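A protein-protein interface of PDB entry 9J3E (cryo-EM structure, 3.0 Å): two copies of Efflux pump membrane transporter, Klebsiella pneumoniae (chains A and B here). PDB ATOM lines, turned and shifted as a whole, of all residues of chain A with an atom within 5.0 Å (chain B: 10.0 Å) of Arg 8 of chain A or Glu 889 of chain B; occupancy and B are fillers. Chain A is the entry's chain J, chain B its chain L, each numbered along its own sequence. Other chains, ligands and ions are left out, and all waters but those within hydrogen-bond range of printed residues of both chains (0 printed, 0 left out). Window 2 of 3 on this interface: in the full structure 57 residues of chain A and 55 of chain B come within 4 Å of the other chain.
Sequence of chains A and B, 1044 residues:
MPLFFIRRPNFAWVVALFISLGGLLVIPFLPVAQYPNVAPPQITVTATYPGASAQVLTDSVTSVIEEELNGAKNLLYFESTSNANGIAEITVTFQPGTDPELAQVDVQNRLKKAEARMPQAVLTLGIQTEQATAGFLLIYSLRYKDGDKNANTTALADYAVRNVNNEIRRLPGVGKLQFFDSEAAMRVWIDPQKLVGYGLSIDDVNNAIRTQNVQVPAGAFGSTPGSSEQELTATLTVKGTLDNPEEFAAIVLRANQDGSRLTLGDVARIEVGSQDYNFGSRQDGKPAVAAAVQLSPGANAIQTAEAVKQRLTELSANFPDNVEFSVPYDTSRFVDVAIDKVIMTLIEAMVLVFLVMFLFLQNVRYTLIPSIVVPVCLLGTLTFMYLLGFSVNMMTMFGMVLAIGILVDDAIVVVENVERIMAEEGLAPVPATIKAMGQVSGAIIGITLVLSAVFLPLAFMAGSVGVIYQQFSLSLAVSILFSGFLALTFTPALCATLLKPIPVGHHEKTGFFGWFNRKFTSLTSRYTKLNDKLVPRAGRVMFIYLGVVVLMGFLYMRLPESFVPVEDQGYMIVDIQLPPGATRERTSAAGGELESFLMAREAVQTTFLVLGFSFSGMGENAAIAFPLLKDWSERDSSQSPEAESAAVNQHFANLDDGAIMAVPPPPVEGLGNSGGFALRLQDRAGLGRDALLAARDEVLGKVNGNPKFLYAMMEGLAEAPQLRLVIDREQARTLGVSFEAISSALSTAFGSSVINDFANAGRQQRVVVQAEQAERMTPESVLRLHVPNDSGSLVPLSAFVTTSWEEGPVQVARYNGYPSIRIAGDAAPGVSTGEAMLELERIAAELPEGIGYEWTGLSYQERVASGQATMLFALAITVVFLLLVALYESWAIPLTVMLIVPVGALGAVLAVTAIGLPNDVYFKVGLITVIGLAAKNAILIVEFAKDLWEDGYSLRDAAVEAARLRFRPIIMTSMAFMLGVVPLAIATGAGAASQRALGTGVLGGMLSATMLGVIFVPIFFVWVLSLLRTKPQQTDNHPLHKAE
N of Asn 10 of chain A is in hydrogen-bond range of OE1 of Glu 889 of chain B.
The side-chain carboxylate (OE1) of Glu 889 of chain B lies close to the backbone nitrogen (N) of Pro 9 of chain A, at 3.5 Å.
The side-chain amide nitrogen (ND2) of Asn 10 of chain A lies close to the backbone NH (N) of Ser 890 of chain B (3.3 Å).
The side-chain amide oxygen (OD1) of Asn 10 of chain A lies within hydrogen-bond range of the indole nitrogen (NE1) of Trp 891 of chain B (3.1 Å).
The backbone NH (N) of Ala 892 of chain B sits at hydrogen-bond distance from the side-chain hydroxyl (OG) of Ser 890 of chain B, 3.3 Å away.
Among the printed residues, pairs that only touch across the chains: Arg 8 of chain A with Glu 889 of chain B (3.4 Å), Phe 11 of chain A with Glu 889 of chain B (3.9 Å) and Asn 10 of chain A with Val 885 of chain B (3.98 Å).
Printed residues of chain B within 4 Å of Arg 8 of chain A: Glu 889.
Printed residues of chain A within 4 Å of Ser 890 of chain B: Asn 10 (3.3 Å).
Of the printed residues of chain A, Val 885 of chain B touches Asn 10.
The nearest residue of chain A that does not touch Glu 889 of chain B is Arg 7 of chain A (4.9 Å).
The nearest printed residue of chain B that does not touch Phe 11 of chain A is Ala 886 of chain B (4.6 Å).
Printed residues of chain A that touch a printed residue of chain B: Arg 8, Pro 9, Asn 10 and Phe 11.
Along chain A the printed residues that touch a printed residue of chain B span positions 8 to 11.
Of the 20 printed residues of chain B, 4 touch a printed residue of chain A.
Among the printed residues, 7 pairs touch across the chains.
Among the printed residues, no Asp or Glu carboxylate lies within 4 Å of a Lys or Arg side-chain nitrogen of the other chain.
No position is printed for both chains.
Of the 7 pairs that touch across the chains among the printed residues, none has its exchanged pair printed and touching as well.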
ATOM      1  N   LEU A   3       5.577 -11.918 -19.597  1.00  0.00           N
ATOM      2  CA  LEU A   3       5.648 -13.104 -18.749  1.00  0.00           C
ATOM      3  C   LEU A   3       6.964 -13.140 -17.984  1.00  0.00           C
ATOM      4  O   LEU A   3       7.027 -13.665 -16.868  1.00  0.00           O
ATOM      5  CB  LEU A   3       5.488 -14.392 -19.563  1.00  0.00           C
ATOM      6  CG  LEU A   3       6.516 -14.909 -20.585  1.00  0.00           C
ATOM      7  CD1 LEU A   3       5.967 -16.155 -21.281  1.00  0.00           C
ATOM      8  CD2 LEU A   3       6.946 -13.876 -21.621  1.00  0.00           C
ATOM      9  N   PHE A   4       8.025 -12.583 -18.575  1.00  0.00           N
ATOM     10  CA  PHE A   4       9.319 -12.520 -17.905  1.00  0.00           C
ATOM     11  C   PHE A   4       9.195 -11.870 -16.538  1.00  0.00           C
ATOM     12  O   PHE A   4       9.640 -12.435 -15.532  1.00  0.00           O
ATOM     13  CB  PHE A   4      10.313 -11.757 -18.789  1.00  0.00           C
ATOM     14  CG  PHE A   4      11.718 -11.651 -18.230  1.00  0.00           C
ATOM     15  CD1 PHE A   4      12.168 -12.470 -17.210  1.00  0.00           C
ATOM     16  CD2 PHE A   4      12.598 -10.725 -18.762  1.00  0.00           C
ATOM     17  CE1 PHE A   4      13.454 -12.346 -16.724  1.00  0.00           C
ATOM     18  CE2 PHE A   4      13.879 -10.604 -18.283  1.00  0.00           C
ATOM     19  CZ  PHE A   4      14.308 -11.414 -17.264  1.00  0.00           C
ATOM     20  N   PHE A   5       8.579 -10.697 -16.473  1.00  0.00           N
ATOM     21  CA  PHE A   5       8.386 -10.067 -15.178  1.00  0.00           C
ATOM     22  C   PHE A   5       7.227 -10.658 -14.397  1.00  0.00           C
ATOM     23  O   PHE A   5       7.182 -10.507 -13.172  1.00  0.00           O
ATOM     24  CB  PHE A   5       8.223  -8.562 -15.355  1.00  0.00           C
ATOM     25  CG  PHE A   5       9.486  -7.882 -15.768  1.00  0.00           C
ATOM     26  CD1 PHE A   5      10.344  -7.386 -14.803  1.00  0.00           C
ATOM     27  CD2 PHE A   5       9.857  -7.798 -17.094  1.00  0.00           C
ATOM     28  CE1 PHE A   5      11.518  -6.767 -15.147  1.00  0.00           C
ATOM     29  CE2 PHE A   5      11.043  -7.182 -17.449  1.00  0.00           C
ATOM     30  CZ  PHE A   5      11.872  -6.666 -16.473  1.00  0.00           C
ATOM     31  N   ILE A   6       6.295 -11.345 -15.052  1.00  0.00           N
ATOM     32  CA  ILE A   6       5.257 -12.010 -14.273  1.00  0.00           C
ATOM     33  C   ILE A   6       5.859 -13.124 -13.422  1.00  0.00           C
ATOM     34  O   ILE A   6       5.511 -13.277 -12.247  1.00  0.00           O
ATOM     35  CB  ILE A   6       4.130 -12.517 -15.188  1.00  0.00           C
ATOM     36  CG1 ILE A   6       3.107 -11.406 -15.372  1.00  0.00           C
ATOM     37  CG2 ILE A   6       3.428 -13.701 -14.554  1.00  0.00           C
ATOM     38  CD1 ILE A   6       2.442 -11.030 -14.081  1.00  0.00           C
ATOM     39  N   ARG A   7       6.779 -13.910 -13.992  1.00  0.00           N
ATOM     40  CA  ARG A   7       7.369 -15.020 -13.245  1.00  0.00           C
ATOM     41  C   ARG A   7       8.432 -14.560 -12.256  1.00  0.00           C
ATOM     42  O   ARG A   7       8.740 -15.300 -11.319  1.00  0.00           O
ATOM     43  CB  ARG A   7       7.973 -16.064 -14.186  1.00  0.00           C
ATOM     44  CG  ARG A   7       8.747 -15.511 -15.366  1.00  0.00           C
ATOM     45  CD  ARG A   7       9.014 -16.591 -16.413  1.00  0.00           C
ATOM     46  NE  ARG A   7      10.172 -16.286 -17.245  1.00  0.00           N
ATOM     47  CZ  ARG A   7      10.391 -16.808 -18.445  1.00  0.00           C
ATOM     48  NH1 ARG A   7       9.557 -17.687 -18.979  1.00  0.00           N
ATOM     49  NH2 ARG A   7      11.473 -16.440 -19.124  1.00  0.00           N
ATOM     50  N   ARG A   8       9.013 -13.378 -12.497  1.00  0.00           N
ATOM     51  CA  ARG A   8      10.056 -12.826 -11.588  1.00  0.00           C
ATOM     52  C   ARG A   8       9.585 -11.473 -11.047  1.00  0.00           C
ATOM     53  O   ARG A   8       9.975 -10.437 -11.621  1.00  0.00           O
ATOM     54  CB  ARG A   8      11.397 -12.671 -12.313  1.00  0.00           C
ATOM     55  CG  ARG A   8      11.635 -13.690 -13.416  1.00  0.00           C
ATOM     56  CD  ARG A   8      12.827 -14.592 -13.168  1.00  0.00           C
ATOM     57  NE  ARG A   8      13.271 -15.223 -14.403  1.00  0.00           N
ATOM     58  CZ  ARG A   8      12.831 -16.393 -14.853  1.00  0.00           C
ATOM     59  NH1 ARG A   8      11.932 -17.075 -14.163  1.00  0.00           N
ATOM     60  NH2 ARG A   8      13.296 -16.880 -15.989  1.00  0.00           N
ATOM     61  N   PRO A   9       8.764 -11.437  -9.974  1.00  0.00           N
ATOM     62  CA  PRO A   9       8.244 -10.179  -9.432  1.00  0.00           C
ATOM     63  C   PRO A   9       9.358  -9.268  -8.899  1.00  0.00           C
ATOM     64  O   PRO A   9       9.271  -8.073  -9.108  1.00  0.00           O
ATOM     65  CB  PRO A   9       7.364 -10.627  -8.256  1.00  0.00           C
ATOM     66  CG  PRO A   9       7.028 -12.067  -8.567  1.00  0.00           C
ATOM     67  CD  PRO A   9       8.278 -12.601  -9.232  1.00  0.00           C
ATOM     68  N   ASN A  10      10.357  -9.845  -8.224  1.00  0.00           N
ATOM     69  CA  ASN A  10      11.433  -9.020  -7.611  1.00  0.00           C
ATOM     70  C   ASN A  10      12.189  -8.250  -8.697  1.00  0.00           C
ATOM     71  O   ASN A  10      12.599  -7.117  -8.411  1.00  0.00           O
ATOM     72  CB  ASN A  10      12.357  -9.837  -6.705  1.00  0.00           C
ATOM     73  CG  ASN A  10      11.928  -9.781  -5.256  1.00  0.00           C
ATOM     74  OD1 ASN A  10      11.372  -8.779  -4.811  1.00  0.00           O
ATOM     75  ND2 ASN A  10      12.165 -10.852  -4.518  1.00  0.00           N
ATOM     76  N   PHE A  11      12.367  -8.833  -9.887  1.00  0.00           N
ATOM     77  CA  PHE A  11      13.008  -8.087 -10.964  1.00  0.00           C
ATOM     78  C   PHE A  11      12.263  -6.781 -11.243  1.00  0.00           C
ATOM     79  O   PHE A  11      12.866  -5.700 -11.283  1.00  0.00           O
ATOM     80  CB  PHE A  11      13.086  -8.949 -12.220  1.00  0.00           C
ATOM     81  CG  PHE A  11      14.171  -8.552 -13.188  1.00  0.00           C
ATOM     82  CD1 PHE A  11      14.856  -7.362 -13.033  1.00  0.00           C
ATOM     83  CD2 PHE A  11      14.513  -9.375 -14.246  1.00  0.00           C
ATOM     84  CE1 PHE A  11      15.850  -6.999 -13.917  1.00  0.00           C
ATOM     85  CE2 PHE A  11      15.510  -9.017 -15.135  1.00  0.00           C
ATOM     86  CZ  PHE A  11      16.180  -7.825 -14.967  1.00  0.00           C
ATOM     87  N   ALA A  12      10.949  -6.862 -11.441  1.00  0.00           N
ATOM     88  CA  ALA A  12      10.172  -5.658 -11.699  1.00  0.00           C
ATOM     89  C   ALA A  12      10.197  -4.726 -10.501  1.00  0.00           C
ATOM     90  O   ALA A  12      10.334  -3.503 -10.652  1.00  0.00           O
ATOM     91  CB  ALA A  12       8.735  -6.023 -12.054  1.00  0.00           C
ATOM     92  N   PHE B 881      22.842  -3.746  -2.916  1.00  0.00           N
ATOM     93  CA  PHE B 881      21.684  -4.471  -2.397  1.00  0.00           C
ATOM     94  C   PHE B 881      20.629  -4.659  -3.471  1.00  0.00           C
ATOM     95  O   PHE B 881      20.084  -5.757  -3.636  1.00  0.00           O
ATOM     96  CB  PHE B 881      21.075  -3.735  -1.206  1.00  0.00           C
ATOM     97  CG  PHE B 881      19.817  -4.376  -0.676  1.00  0.00           C
ATOM     98  CD1 PHE B 881      19.859  -5.573   0.016  1.00  0.00           C
ATOM     99  CD2 PHE B 881      18.588  -3.772  -0.868  1.00  0.00           C
ATOM    100  CE1 PHE B 881      18.706  -6.154   0.501  1.00  0.00           C
ATOM    101  CE2 PHE B 881      17.430  -4.350  -0.384  1.00  0.00           C
ATOM    102  CZ  PHE B 881      17.492  -5.542   0.302  1.00  0.00           C
ATOM    103  N   LEU B 882      20.307  -3.587  -4.191  1.00  0.00           N
ATOM    104  CA  LEU B 882      19.225  -3.670  -5.165  1.00  0.00           C
ATOM    105  C   LEU B 882      19.588  -4.599  -6.318  1.00  0.00           C
ATOM    106  O   LEU B 882      18.754  -5.382  -6.788  1.00  0.00           O
ATOM    107  CB  LEU B 882      18.881  -2.274  -5.665  1.00  0.00           C
ATOM    108  CG  LEU B 882      17.601  -1.739  -5.037  1.00  0.00           C
ATOM    109  CD1 LEU B 882      16.449  -2.666  -5.345  1.00  0.00           C
ATOM    110  CD2 LEU B 882      17.779  -1.590  -3.540  1.00  0.00           C
ATOM    111  N   LEU B 883      20.836  -4.541  -6.773  1.00  0.00           N
ATOM    112  CA  LEU B 883      21.287  -5.467  -7.805  1.00  0.00           C
ATOM    113  C   LEU B 883      21.204  -6.903  -7.319  1.00  0.00           C
ATOM    114  O   LEU B 883      20.846  -7.811  -8.081  1.00  0.00           O
ATOM    115  CB  LEU B 883      22.714  -5.129  -8.206  1.00  0.00           C
ATOM    116  CG  LEU B 883      22.768  -3.832  -8.988  1.00  0.00           C
ATOM    117  CD1 LEU B 883      24.199  -3.480  -9.297  1.00  0.00           C
ATOM    118  CD2 LEU B 883      21.945  -3.996 -10.243  1.00  0.00           C
ATOM    119  N   LEU B 884      21.530  -7.125  -6.050  1.00  0.00           N
ATOM    120  CA  LEU B 884      21.547  -8.480  -5.522  1.00  0.00           C
ATOM    121  C   LEU B 884      20.135  -9.037  -5.395  1.00  0.00           C
ATOM    122  O   LEU B 884      19.900 -10.213  -5.693  1.00  0.00           O
ATOM    123  CB  LEU B 884      22.279  -8.475  -4.189  1.00  0.00           C
ATOM    124  CG  LEU B 884      23.774  -8.499  -4.492  1.00  0.00           C
ATOM    125  CD1 LEU B 884      24.608  -8.472  -3.241  1.00  0.00           C
ATOM    126  CD2 LEU B 884      24.110  -9.714  -5.333  1.00  0.00           C
ATOM    127  N   VAL B 885      19.177  -8.208  -4.971  1.00  0.00           N
ATOM    128  CA  VAL B 885      17.794  -8.682  -4.955  1.00  0.00           C
ATOM    129  C   VAL B 885      17.290  -8.913  -6.368  1.00  0.00           C
ATOM    130  O   VAL B 885      16.527  -9.855  -6.613  1.00  0.00           O
ATOM    131  CB  VAL B 885      16.871  -7.742  -4.149  1.00  0.00           C
ATOM    132  CG1 VAL B 885      17.163  -6.323  -4.432  1.00  0.00           C
ATOM    133  CG2 VAL B 885      15.408  -8.005  -4.481  1.00  0.00           C
ATOM    134  N   ALA B 886      17.722  -8.098  -7.329  1.00  0.00           N
ATOM    135  CA  ALA B 886      17.346  -8.361  -8.713  1.00  0.00           C
ATOM    136  C   ALA B 886      17.837  -9.728  -9.157  1.00  0.00           C
ATOM    137  O   ALA B 886      17.075 -10.529  -9.706  1.00  0.00           O
ATOM    138  CB  ALA B 886      17.904  -7.275  -9.628  1.00  0.00           C
ATOM    139  N   LEU B 887      19.109 -10.021  -8.906  1.00  0.00           N
ATOM    140  CA  LEU B 887      19.692 -11.237  -9.458  1.00  0.00           C
ATOM    141  C   LEU B 887      19.175 -12.473  -8.732  1.00  0.00           C
ATOM    142  O   LEU B 887      18.890 -13.495  -9.366  1.00  0.00           O
ATOM    143  CB  LEU B 887      21.218 -11.152  -9.397  1.00  0.00           C
ATOM    144  CG  LEU B 887      22.067 -12.008 -10.347  1.00  0.00           C
ATOM    145  CD1 LEU B 887      21.972 -13.500 -10.077  1.00  0.00           C
ATOM    146  CD2 LEU B 887      21.691 -11.706 -11.794  1.00  0.00           C
ATOM    147  N   TYR B 888      19.030 -12.400  -7.412  1.00  0.00           N
ATOM    148  CA  TYR B 888      18.671 -13.564  -6.612  1.00  0.00           C
ATOM    149  C   TYR B 888      17.173 -13.771  -6.473  1.00  0.00           C
ATOM    150  O   TYR B 888      16.764 -14.751  -5.843  1.00  0.00           O
ATOM    151  CB  TYR B 888      19.299 -13.459  -5.224  1.00  0.00           C
ATOM    152  CG  TYR B 888      20.785 -13.621  -5.275  1.00  0.00           C
ATOM    153  CD1 TYR B 888      21.355 -14.553  -6.118  1.00  0.00           C
ATOM    154  CD2 TYR B 888      21.616 -12.827  -4.510  1.00  0.00           C
ATOM    155  CE1 TYR B 888      22.706 -14.706  -6.186  1.00  0.00           C
ATOM    156  CE2 TYR B 888      22.973 -12.978  -4.568  1.00  0.00           C
ATOM    157  CZ  TYR B 888      23.512 -13.917  -5.411  1.00  0.00           C
ATOM    158  OH  TYR B 888      24.869 -14.071  -5.483  1.00  0.00           O
ATOM    159  N   GLU B 889      16.353 -12.887  -7.035  1.00  0.00           N
ATOM    160  CA  GLU B 889      14.903 -13.046  -7.003  1.00  0.00           C
ATOM    161  C   GLU B 889      14.450 -13.265  -5.560  1.00  0.00           C
ATOM    162  O   GLU B 889      13.640 -14.141  -5.255  1.00  0.00           O
ATOM    163  CB  GLU B 889      14.473 -14.194  -7.924  1.00  0.00           C
ATOM    164  CG  GLU B 889      12.968 -14.484  -8.061  1.00  0.00           C
ATOM    165  CD  GLU B 889      12.087 -13.276  -7.793  1.00  0.00           C
ATOM    166  OE1 GLU B 889      11.858 -12.492  -8.736  1.00  0.00           O
ATOM    167  OE2 GLU B 889      11.604 -13.118  -6.655  1.00  0.00           O
ATOM    168  N   SER B 890      15.030 -12.488  -4.650  1.00  0.00           N
ATOM    169  CA  SER B 890      14.784 -12.658  -3.226  1.00  0.00           C
ATOM    170  C   SER B 890      15.390 -11.485  -2.479  1.00  0.00           C
ATOM    171  O   SER B 890      16.091 -10.657  -3.057  1.00  0.00           O
ATOM    172  CB  SER B 890      15.374 -13.969  -2.704  1.00  0.00           C
ATOM    173  OG  SER B 890      15.323 -14.015  -1.289  1.00  0.00           O
ATOM    174  N   TRP B 891      15.118 -11.435  -1.177  1.00  0.00           N
ATOM    175  CA  TRP B 891      15.729 -10.446  -0.299  1.00  0.00           C
ATOM    176  C   TRP B 891      16.709 -11.072   0.678  1.00  0.00           C
ATOM    177  O   TRP B 891      17.806 -10.532   0.894  1.00  0.00           O
ATOM    178  CB  TRP B 891      14.649  -9.694   0.476  1.00  0.00           C
ATOM    179  CG  TRP B 891      13.623  -9.109  -0.416  1.00  0.00           C
ATOM    180  CD1 TRP B 891      12.505  -9.725  -0.879  1.00  0.00           C
ATOM    181  CD2 TRP B 891      13.633  -7.803  -0.997  1.00  0.00           C
ATOM    182  NE1 TRP B 891      11.801  -8.878  -1.695  1.00  0.00           N
ATOM    183  CE2 TRP B 891      12.475  -7.690  -1.787  1.00  0.00           C
ATOM    184  CE3 TRP B 891      14.503  -6.714  -0.920  1.00  0.00           C
ATOM    185  CZ2 TRP B 891      12.164  -6.533  -2.495  1.00  0.00           C
ATOM    186  CZ3 TRP B 891      14.193  -5.567  -1.624  1.00  0.00           C
ATOM    187  CH2 TRP B 891      13.034  -5.486  -2.401  1.00  0.00           C
ATOM    188  N   ALA B 892      16.341 -12.224   1.241  1.00  0.00           N
ATOM    189  CA  ALA B 892      17.188 -12.866   2.233  1.00  0.00           C
ATOM    190  C   ALA B 892      18.570 -13.154   1.671  1.00  0.00           C
ATOM    191  O   ALA B 892      19.577 -12.871   2.324  1.00  0.00           O
ATOM    192  CB  ALA B 892      16.533 -14.153   2.728  1.00  0.00           C
ATOM    193  N   ILE B 893      18.635 -13.716   0.460  1.00  0.00           N
ATOM    194  CA  ILE B 893      19.938 -13.999  -0.151  1.00  0.00           C
ATOM    195  C   ILE B 893      20.738 -12.723  -0.360  1.00  0.00           C
ATOM    196  O   ILE B 893      21.958 -12.735  -0.119  1.00  0.00           O
ATOM    197  CB  ILE B 893      19.754 -14.826  -1.435  1.00  0.00           C
ATOM    198  CG1 ILE B 893      19.110 -16.182  -1.138  1.00  0.00           C
ATOM    199  CG2 ILE B 893      21.081 -15.081  -2.102  1.00  0.00           C
ATOM    200  CD1 ILE B 893      17.602 -16.173  -1.043  1.00  0.00           C
ATOM    201  N   PRO B 894      20.160 -11.613  -0.830  1.00  0.00           N
ATOM    202  CA  PRO B 894      20.923 -10.356  -0.845  1.00  0.00           C
ATOM    203  C   PRO B 894      21.502  -9.950   0.495  1.00  0.00           C
ATOM    204  O   PRO B 894      22.694  -9.628   0.541  1.00  0.00           O
ATOM    205  CB  PRO B 894      19.899  -9.335  -1.346  1.00  0.00           C
ATOM    206  CG  PRO B 894      18.970 -10.111  -2.137  1.00  0.00           C
ATOM    207  CD  PRO B 894      18.959 -11.521  -1.673  1.00  0.00           C
ATOM    208  N   LYS B 946      22.646 -21.544  -3.737  1.00  0.00           N
ATOM    209  CA  LYS B 946      21.241 -21.401  -4.097  1.00  0.00           C
ATOM    210  C   LYS B 946      20.833 -22.424  -5.149  1.00  0.00           C
ATOM    211  O   LYS B 946      19.734 -22.987  -5.086  1.00  0.00           O
ATOM    212  CB  LYS B 946      20.996 -19.980  -4.599  1.00  0.00           C
ATOM    213  CG  LYS B 946      19.599 -19.691  -5.101  1.00  0.00           C
ATOM    214  CD  LYS B 946      18.542 -20.128  -4.120  1.00  0.00           C
ATOM    215  CE  LYS B 946      17.324 -19.231  -4.218  1.00  0.00           C
ATOM    216  NZ  LYS B 946      17.374 -18.370  -5.430  1.00  0.00           N
ATOM    217  N   TRP B 949      20.421 -25.714  -3.401  1.00  0.00           N
ATOM    218  CA  TRP B 949      19.276 -25.724  -2.500  1.00  0.00           C
ATOM    219  C   TRP B 949      17.962 -25.566  -3.247  1.00  0.00           C
ATOM    220  O   TRP B 949      16.891 -25.751  -2.662  1.00  0.00           O
ATOM    221  CB  TRP B 949      19.476 -24.659  -1.425  1.00  0.00           C
ATOM    222  CG  TRP B 949      18.294 -24.344  -0.574  1.00  0.00           C
ATOM    223  CD1 TRP B 949      17.879 -25.015   0.534  1.00  0.00           C
ATOM    224  CD2 TRP B 949      17.478 -23.173  -0.658  1.00  0.00           C
ATOM    225  NE1 TRP B 949      16.792 -24.386   1.090  1.00  0.00           N
ATOM    226  CE2 TRP B 949      16.534 -23.245   0.381  1.00  0.00           C
ATOM    227  CE3 TRP B 949      17.432 -22.089  -1.535  1.00  0.00           C
ATOM    228  CZ2 TRP B 949      15.557 -22.274   0.566  1.00  0.00           C
ATOM    229  CZ3 TRP B 949      16.462 -21.130  -1.349  1.00  0.00           C
ATOM    230  CH2 TRP B 949      15.540 -21.226  -0.307  1.00  0.00           C
ATOM    231  N   GLU B 950      18.014 -25.234  -4.530  1.00  0.00           N
ATOM    232  CA  GLU B 950      16.830 -25.372  -5.363  1.00  0.00           C
ATOM    233  C   GLU B 950      16.715 -26.752  -5.996  1.00  0.00           C
ATOM    234  O   GLU B 950      15.644 -27.095  -6.506  1.00  0.00           O
ATOM    235  CB  GLU B 950      16.817 -24.299  -6.452  1.00  0.00           C
ATOM    236  CG  GLU B 950      16.342 -22.942  -5.965  1.00  0.00           C
ATOM    237  CD  GLU B 950      16.302 -21.906  -7.067  1.00  0.00           C
ATOM    238  OE1 GLU B 950      16.903 -22.146  -8.135  1.00  0.00           O
ATOM    239  OE2 GLU B 950      15.660 -20.854  -6.867  1.00  0.00           O
ATOM    240  N   THR B1030      13.642 -18.890   5.018  1.00  0.00           N
ATOM    241  CA  THR B1030      13.478 -18.830   3.573  1.00  0.00           C
ATOM    242  C   THR B1030      13.140 -20.202   3.002  1.00  0.00           C
ATOM    243  O   THR B1030      13.548 -21.236   3.537  1.00  0.00           O
ATOM    244  CB  THR B1030      14.748 -18.292   2.921  1.00  0.00           C
ATOM    245  OG1 THR B1030      15.322 -17.283   3.760  1.00  0.00           O
ATOM    246  CG2 THR B1030      14.436 -17.696   1.560  1.00  0.00           C
ATOM    247  N   LYS B1031      12.386 -20.201   1.904  1.00  0.00           N
ATOM    248  CA  LYS B1031      11.909 -21.398   1.240  1.00  0.00           C
ATOM    249  C   LYS B1031      12.345 -21.404  -0.222  1.00  0.00           C
ATOM    250  O   LYS B1031      12.476 -20.343  -0.838  1.00  0.00           O
ATOM    251  CB  LYS B1031      10.379 -21.472   1.315  1.00  0.00           C
ATOM    252  CG  LYS B1031       9.852 -21.703   2.721  1.00  0.00           C
ATOM    253  CD  LYS B1031       8.346 -21.904   2.738  1.00  0.00           C
ATOM    254  CE  LYS B1031       7.853 -22.206   4.145  1.00  0.00           C
ATOM    255  NZ  LYS B1031       6.383 -22.443   4.189  1.00  0.00           N
ATOM    256  N   PRO B1032      12.594 -22.582  -0.810  1.00  0.00           N
ATOM    257  CA  PRO B1032      13.001 -22.647  -2.217  1.00  0.00           C
ATOM    258  C   PRO B1032      11.821 -22.504  -3.168  1.00  0.00           C
ATOM    259  O   PRO B1032      10.695 -22.369  -2.689  1.00  0.00           O
ATOM    260  CB  PRO B1032      13.627 -24.034  -2.332  1.00  0.00           C
ATOM    261  CG  PRO B1032      12.908 -24.841  -1.316  1.00  0.00           C
ATOM    262  CD  PRO B1032      12.564 -23.912  -0.181  1.00  0.00           C
